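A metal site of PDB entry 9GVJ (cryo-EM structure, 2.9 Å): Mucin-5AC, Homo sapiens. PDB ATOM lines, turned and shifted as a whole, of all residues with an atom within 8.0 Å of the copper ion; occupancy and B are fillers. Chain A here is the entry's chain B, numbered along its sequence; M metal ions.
A ring nitrogen (ND1) of His 340 sits at hydrogen-bond distance from the backbone carbonyl oxygen (O) of Thr 292 (3.5 Å). A ring nitrogen (ND1) of His 49 is in hydrogen-bond range of the backbone carbonyl oxygen of Pro 47. N of Glu 171 is in hydrogen-bond range of O of Val 159, 2.9 Å away.
Within 4 Å of the copper ion: His 49, Glu 171, His 293 and His 340. Along chain A the residues within 4 Å of the copper ion span positions 49 to 340. The nearest printed residue that does not touch the copper ion is Val 53 (4.5 Å).
The copper ion is bound by NE2 of His 340 (2.2 Å), NE2 of His 49 (2.2 Å), ND1 of His 293 (2.2 Å) and OE1 of Glu 171 (2.5 Å).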
ATOM      1  N   PRO A  47       1.665 -11.366 -17.864  1.00  0.00           N
ATOM      2  CA  PRO A  47       1.888 -12.799 -18.104  1.00  0.00           C
ATOM      3  C   PRO A  47       0.881 -13.703 -17.418  1.00  0.00           C
ATOM      4  O   PRO A  47       0.699 -14.844 -17.859  1.00  0.00           O
ATOM      5  CB  PRO A  47       3.308 -13.023 -17.566  1.00  0.00           C
ATOM      6  CG  PRO A  47       3.498 -11.947 -16.555  1.00  0.00           C
ATOM      7  CD  PRO A  47       2.757 -10.748 -17.096  1.00  0.00           C
ATOM      8  N   ALA A  48       0.224 -13.252 -16.351  1.00  0.00           N
ATOM      9  CA  ALA A  48      -0.755 -14.070 -15.648  1.00  0.00           C
ATOM     10  C   ALA A  48      -1.961 -14.294 -16.556  1.00  0.00           C
ATOM     11  O   ALA A  48      -2.722 -13.370 -16.840  1.00  0.00           O
ATOM     12  CB  ALA A  48      -1.176 -13.392 -14.343  1.00  0.00           C
ATOM     13  N   HIS A  49      -2.130 -15.530 -17.011  1.00  0.00           N
ATOM     14  CA  HIS A  49      -3.168 -15.863 -17.987  1.00  0.00           C
ATOM     15  C   HIS A  49      -3.877 -17.156 -17.590  1.00  0.00           C
ATOM     16  O   HIS A  49      -4.175 -18.006 -18.442  1.00  0.00           O
ATOM     17  CB  HIS A  49      -2.583 -15.975 -19.398  1.00  0.00           C
ATOM     18  CG  HIS A  49      -1.453 -16.951 -19.505  1.00  0.00           C
ATOM     19  ND1 HIS A  49      -0.132 -16.561 -19.414  1.00  0.00           N
ATOM     20  CD2 HIS A  49      -1.438 -18.288 -19.706  1.00  0.00           C
ATOM     21  CE1 HIS A  49       0.643 -17.617 -19.554  1.00  0.00           C
ATOM     22  NE2 HIS A  49      -0.126 -18.685 -19.733  1.00  0.00           N
ATOM     23  N   ASN A  50      -4.177 -17.319 -16.302  1.00  0.00           N
ATOM     24  CA  ASN A  50      -4.973 -18.458 -15.868  1.00  0.00           C
ATOM     25  C   ASN A  50      -6.404 -18.376 -16.370  1.00  0.00           C
ATOM     26  O   ASN A  50      -7.119 -19.384 -16.341  1.00  0.00           O
ATOM     27  CB  ASN A  50      -4.966 -18.568 -14.345  1.00  0.00           C
ATOM     28  CG  ASN A  50      -3.601 -18.275 -13.749  1.00  0.00           C
ATOM     29  OD1 ASN A  50      -3.313 -17.135 -13.381  1.00  0.00           O
ATOM     30  ND2 ASN A  50      -2.767 -19.296 -13.655  1.00  0.00           N
ATOM     31  N   ARG A  52      -7.322 -18.026 -19.414  1.00  0.00           N
ATOM     32  CA  ARG A  52      -7.401 -18.701 -20.700  1.00  0.00           C
ATOM     33  C   ARG A  52      -7.114 -20.182 -20.600  1.00  0.00           C
ATOM     34  O   ARG A  52      -6.954 -20.850 -21.625  1.00  0.00           O
ATOM     35  CB  ARG A  52      -6.438 -18.055 -21.699  1.00  0.00           C
ATOM     36  CG  ARG A  52      -6.516 -16.533 -21.753  1.00  0.00           C
ATOM     37  CD  ARG A  52      -5.361 -15.950 -22.546  1.00  0.00           C
ATOM     38  NE  ARG A  52      -4.742 -16.952 -23.419  1.00  0.00           N
ATOM     39  CZ  ARG A  52      -3.445 -17.222 -23.452  1.00  0.00           C
ATOM     40  NH1 ARG A  52      -2.584 -16.574 -22.685  1.00  0.00           N
ATOM     41  NH2 ARG A  52      -3.003 -18.155 -24.286  1.00  0.00           N
ATOM     42  N   VAL A  53      -7.035 -20.724 -19.384  1.00  0.00           N
ATOM     43  CA  VAL A  53      -6.652 -22.114 -19.151  1.00  0.00           C
ATOM     44  C   VAL A  53      -7.756 -22.808 -18.373  1.00  0.00           C
ATOM     45  O   VAL A  53      -8.219 -22.285 -17.353  1.00  0.00           O
ATOM     46  CB  VAL A  53      -5.312 -22.208 -18.408  1.00  0.00           C
ATOM     47  CG1 VAL A  53      -4.999 -23.665 -18.060  1.00  0.00           C
ATOM     48  CG2 VAL A  53      -4.194 -21.596 -19.229  1.00  0.00           C
ATOM     49  N   VAL A 159      -4.450 -25.240 -27.517  1.00  0.00           N
ATOM     50  CA  VAL A 159      -3.479 -26.229 -27.085  1.00  0.00           C
ATOM     51  C   VAL A 159      -4.162 -27.176 -26.111  1.00  0.00           C
ATOM     52  O   VAL A 159      -4.771 -26.725 -25.136  1.00  0.00           O
ATOM     53  CB  VAL A 159      -2.241 -25.594 -26.435  1.00  0.00           C
ATOM     54  CG1 VAL A 159      -1.035 -26.527 -26.553  1.00  0.00           C
ATOM     55  CG2 VAL A 159      -1.929 -24.226 -27.048  1.00  0.00           C
ATOM     56  N   MET A 161      -3.318 -30.609 -23.672  1.00  0.00           N
ATOM     57  CA  MET A 161      -2.242 -31.391 -23.082  1.00  0.00           C
ATOM     58  C   MET A 161      -2.860 -32.487 -22.218  1.00  0.00           C
ATOM     59  O   MET A 161      -3.495 -32.182 -21.192  1.00  0.00           O
ATOM     60  CB  MET A 161      -1.297 -30.521 -22.261  1.00  0.00           C
ATOM     61  CG  MET A 161      -0.215 -29.851 -23.079  1.00  0.00           C
ATOM     62  SD  MET A 161       1.371 -29.810 -22.225  1.00  0.00           S
ATOM     63  CE  MET A 161       1.250 -28.242 -21.370  1.00  0.00           C
ATOM     64  N   LEU A 169      -5.444 -30.547 -19.808  1.00  0.00           N
ATOM     65  CA  LEU A 169      -5.334 -29.097 -19.742  1.00  0.00           C
ATOM     66  C   LEU A 169      -5.598 -28.507 -21.117  1.00  0.00           C
ATOM     67  O   LEU A 169      -5.269 -29.115 -22.144  1.00  0.00           O
ATOM     68  CB  LEU A 169      -3.949 -28.660 -19.239  1.00  0.00           C
ATOM     69  CG  LEU A 169      -3.830 -27.236 -18.695  1.00  0.00           C
ATOM     70  CD1 LEU A 169      -3.118 -27.247 -17.356  1.00  0.00           C
ATOM     71  CD2 LEU A 169      -3.098 -26.350 -19.693  1.00  0.00           C
ATOM     72  N   LEU A 170      -6.191 -27.311 -21.142  1.00  0.00           N
ATOM     73  CA  LEU A 170      -6.594 -26.667 -22.390  1.00  0.00           C
ATOM     74  C   LEU A 170      -6.294 -25.176 -22.314  1.00  0.00           C
ATOM     75  O   LEU A 170      -6.854 -24.470 -21.478  1.00  0.00           O
ATOM     76  CB  LEU A 170      -8.080 -26.908 -22.670  1.00  0.00           C
ATOM     77  CG  LEU A 170      -8.620 -26.327 -23.977  1.00  0.00           C
ATOM     78  CD1 LEU A 170      -8.036 -27.077 -25.164  1.00  0.00           C
ATOM     79  CD2 LEU A 170     -10.134 -26.382 -24.002  1.00  0.00           C
ATOM     80  N   GLU A 171      -5.415 -24.715 -23.201  1.00  0.00           N
ATOM     81  CA  GLU A 171      -5.158 -23.300 -23.402  1.00  0.00           C
ATOM     82  C   GLU A 171      -5.945 -22.829 -24.624  1.00  0.00           C
ATOM     83  O   GLU A 171      -5.856 -23.432 -25.699  1.00  0.00           O
ATOM     84  CB  GLU A 171      -3.672 -23.022 -23.615  1.00  0.00           C
ATOM     85  CG  GLU A 171      -2.837 -22.986 -22.350  1.00  0.00           C
ATOM     86  CD  GLU A 171      -1.363 -23.109 -22.650  1.00  0.00           C
ATOM     87  OE1 GLU A 171      -0.544 -22.631 -21.829  1.00  0.00           O
ATOM     88  OE2 GLU A 171      -1.010 -23.683 -23.696  1.00  0.00           O
ATOM     89  N   ARG A 289       1.345 -26.335 -12.152  1.00  0.00           N
ATOM     90  CA  ARG A 289       0.991 -25.965 -13.518  1.00  0.00           C
ATOM     91  C   ARG A 289       0.296 -24.613 -13.566  1.00  0.00           C
ATOM     92  O   ARG A 289       0.609 -23.776 -14.417  1.00  0.00           O
ATOM     93  CB  ARG A 289       0.099 -27.045 -14.131  1.00  0.00           C
ATOM     94  CG  ARG A 289       0.583 -27.590 -15.462  1.00  0.00           C
ATOM     95  CD  ARG A 289       0.402 -29.096 -15.523  1.00  0.00           C
ATOM     96  NE  ARG A 289      -0.827 -29.521 -14.851  1.00  0.00           N
ATOM     97  CZ  ARG A 289      -1.021 -30.723 -14.330  1.00  0.00           C
ATOM     98  NH1 ARG A 289      -0.084 -31.651 -14.383  1.00  0.00           N
ATOM     99  NH2 ARG A 289      -2.186 -30.989 -13.746  1.00  0.00           N
ATOM    100  N   GLN A 290      -0.646 -24.387 -12.648  1.00  0.00           N
ATOM    101  CA  GLN A 290      -1.344 -23.114 -12.605  1.00  0.00           C
ATOM    102  C   GLN A 290      -0.397 -21.967 -12.244  1.00  0.00           C
ATOM    103  O   GLN A 290      -0.529 -20.850 -12.759  1.00  0.00           O
ATOM    104  CB  GLN A 290      -2.505 -23.186 -11.614  1.00  0.00           C
ATOM    105  CG  GLN A 290      -3.574 -24.189 -11.989  1.00  0.00           C
ATOM    106  CD  GLN A 290      -4.207 -23.900 -13.333  1.00  0.00           C
ATOM    107  OE1 GLN A 290      -4.379 -22.743 -13.728  1.00  0.00           O
ATOM    108  NE2 GLN A 290      -4.556 -24.956 -14.069  1.00  0.00           N
ATOM    109  N   THR A 292       2.818 -21.882 -13.014  1.00  0.00           N
ATOM    110  CA  THR A 292       3.560 -21.606 -14.243  1.00  0.00           C
ATOM    111  C   THR A 292       2.714 -20.813 -15.233  1.00  0.00           C
ATOM    112  O   THR A 292       3.221 -19.907 -15.900  1.00  0.00           O
ATOM    113  CB  THR A 292       4.028 -22.913 -14.894  1.00  0.00           C
ATOM    114  OG1 THR A 292       2.898 -23.720 -15.232  1.00  0.00           O
ATOM    115  CG2 THR A 292       4.944 -23.681 -13.955  1.00  0.00           C
ATOM    116  N   HIS A 293       1.422 -21.138 -15.333  1.00  0.00           N
ATOM    117  CA  HIS A 293       0.530 -20.396 -16.224  1.00  0.00           C
ATOM    118  C   HIS A 293       0.258 -18.981 -15.725  1.00  0.00           C
ATOM    119  O   HIS A 293      -0.172 -18.141 -16.517  1.00  0.00           O
ATOM    120  CB  HIS A 293      -0.789 -21.144 -16.394  1.00  0.00           C
ATOM    121  CG  HIS A 293      -0.682 -22.371 -17.239  1.00  0.00           C
ATOM    122  ND1 HIS A 293      -0.170 -22.344 -18.524  1.00  0.00           N
ATOM    123  CD2 HIS A 293      -1.017 -23.654 -16.998  1.00  0.00           C
ATOM    124  CE1 HIS A 293      -0.194 -23.569 -19.024  1.00  0.00           C
ATOM    125  NE2 HIS A 293      -0.702 -24.384 -18.121  1.00  0.00           N
ATOM    126  N   ALA A 294       0.507 -18.703 -14.453  1.00  0.00           N
ATOM    127  CA  ALA A 294       0.262 -17.396 -13.864  1.00  0.00           C
ATOM    128  C   ALA A 294       1.486 -16.487 -13.904  1.00  0.00           C
ATOM    129  O   ALA A 294       1.446 -15.390 -13.336  1.00  0.00           O
ATOM    130  CB  ALA A 294      -0.217 -17.541 -12.415  1.00  0.00           C
ATOM    131  N   GLY A 295       2.561 -16.915 -14.553  1.00  0.00           N
ATOM    132  CA  GLY A 295       3.792 -16.145 -14.585  1.00  0.00           C
ATOM    133  C   GLY A 295       4.731 -16.367 -13.424  1.00  0.00           C
ATOM    134  O   GLY A 295       5.745 -15.672 -13.346  1.00  0.00           O
ATOM    135  N   ASP A 339       7.339 -18.932 -24.865  1.00  0.00           N
ATOM    136  CA  ASP A 339       6.419 -19.516 -23.896  1.00  0.00           C
ATOM    137  C   ASP A 339       7.033 -19.499 -22.501  1.00  0.00           C
ATOM    138  O   ASP A 339       8.253 -19.480 -22.320  1.00  0.00           O
ATOM    139  CB  ASP A 339       6.050 -20.945 -24.293  1.00  0.00           C
ATOM    140  CG  ASP A 339       5.910 -21.120 -25.791  1.00  0.00           C
ATOM    141  OD1 ASP A 339       5.137 -20.350 -26.409  1.00  0.00           O
ATOM    142  OD2 ASP A 339       6.573 -22.016 -26.355  1.00  0.00           O
ATOM    143  N   HIS A 340       6.163 -19.518 -21.492  1.00  0.00           N
ATOM    144  CA  HIS A 340       6.607 -19.513 -20.117  1.00  0.00           C
ATOM    145  C   HIS A 340       7.204 -20.871 -19.750  1.00  0.00           C
ATOM    146  O   HIS A 340       7.089 -21.857 -20.486  1.00  0.00           O
ATOM    147  CB  HIS A 340       5.449 -19.171 -19.178  1.00  0.00           C
ATOM    148  CG  HIS A 340       4.235 -20.025 -19.383  1.00  0.00           C
ATOM    149  ND1 HIS A 340       4.147 -21.322 -18.943  1.00  0.00           N
ATOM    150  CD2 HIS A 340       3.056 -19.755 -19.997  1.00  0.00           C
ATOM    151  CE1 HIS A 340       2.971 -21.819 -19.268  1.00  0.00           C
ATOM    152  NE2 HIS A 340       2.289 -20.891 -19.907  1.00  0.00           N
ATOM    153  N   CYS A 341       7.863 -20.913 -18.588  1.00  0.00           N
ATOM    154  CA  CYS A 341       8.507 -22.135 -18.126  1.00  0.00           C
ATOM    155  C   CYS A 341       7.471 -23.216 -17.835  1.00  0.00           C
ATOM    156  O   CYS A 341       6.347 -22.936 -17.394  1.00  0.00           O
ATOM    157  CB  CYS A 341       9.342 -21.859 -16.892  1.00  0.00           C
ATOM    158  SG  CYS A 341       8.411 -21.735 -15.349  1.00  0.00           S
ATOM    159  N   VAL A 342       7.857 -24.470 -18.097  1.00  0.00           N
ATOM    160  CA  VAL A 342       6.984 -25.617 -17.902  1.00  0.00           C
ATOM    161  C   VAL A 342       7.722 -26.656 -17.057  1.00  0.00           C
ATOM    162  O   VAL A 342       8.915 -26.523 -16.780  1.00  0.00           O
ATOM    163  CB  VAL A 342       6.527 -26.242 -19.228  1.00  0.00           C
ATOM    164  CG1 VAL A 342       5.794 -25.215 -20.079  1.00  0.00           C
ATOM    165  CG2 VAL A 342       7.707 -26.811 -19.986  1.00  0.00           C
HETATM  166 CU    CU M   1       0.098 -20.845 -20.150  1.00  0.00          CU
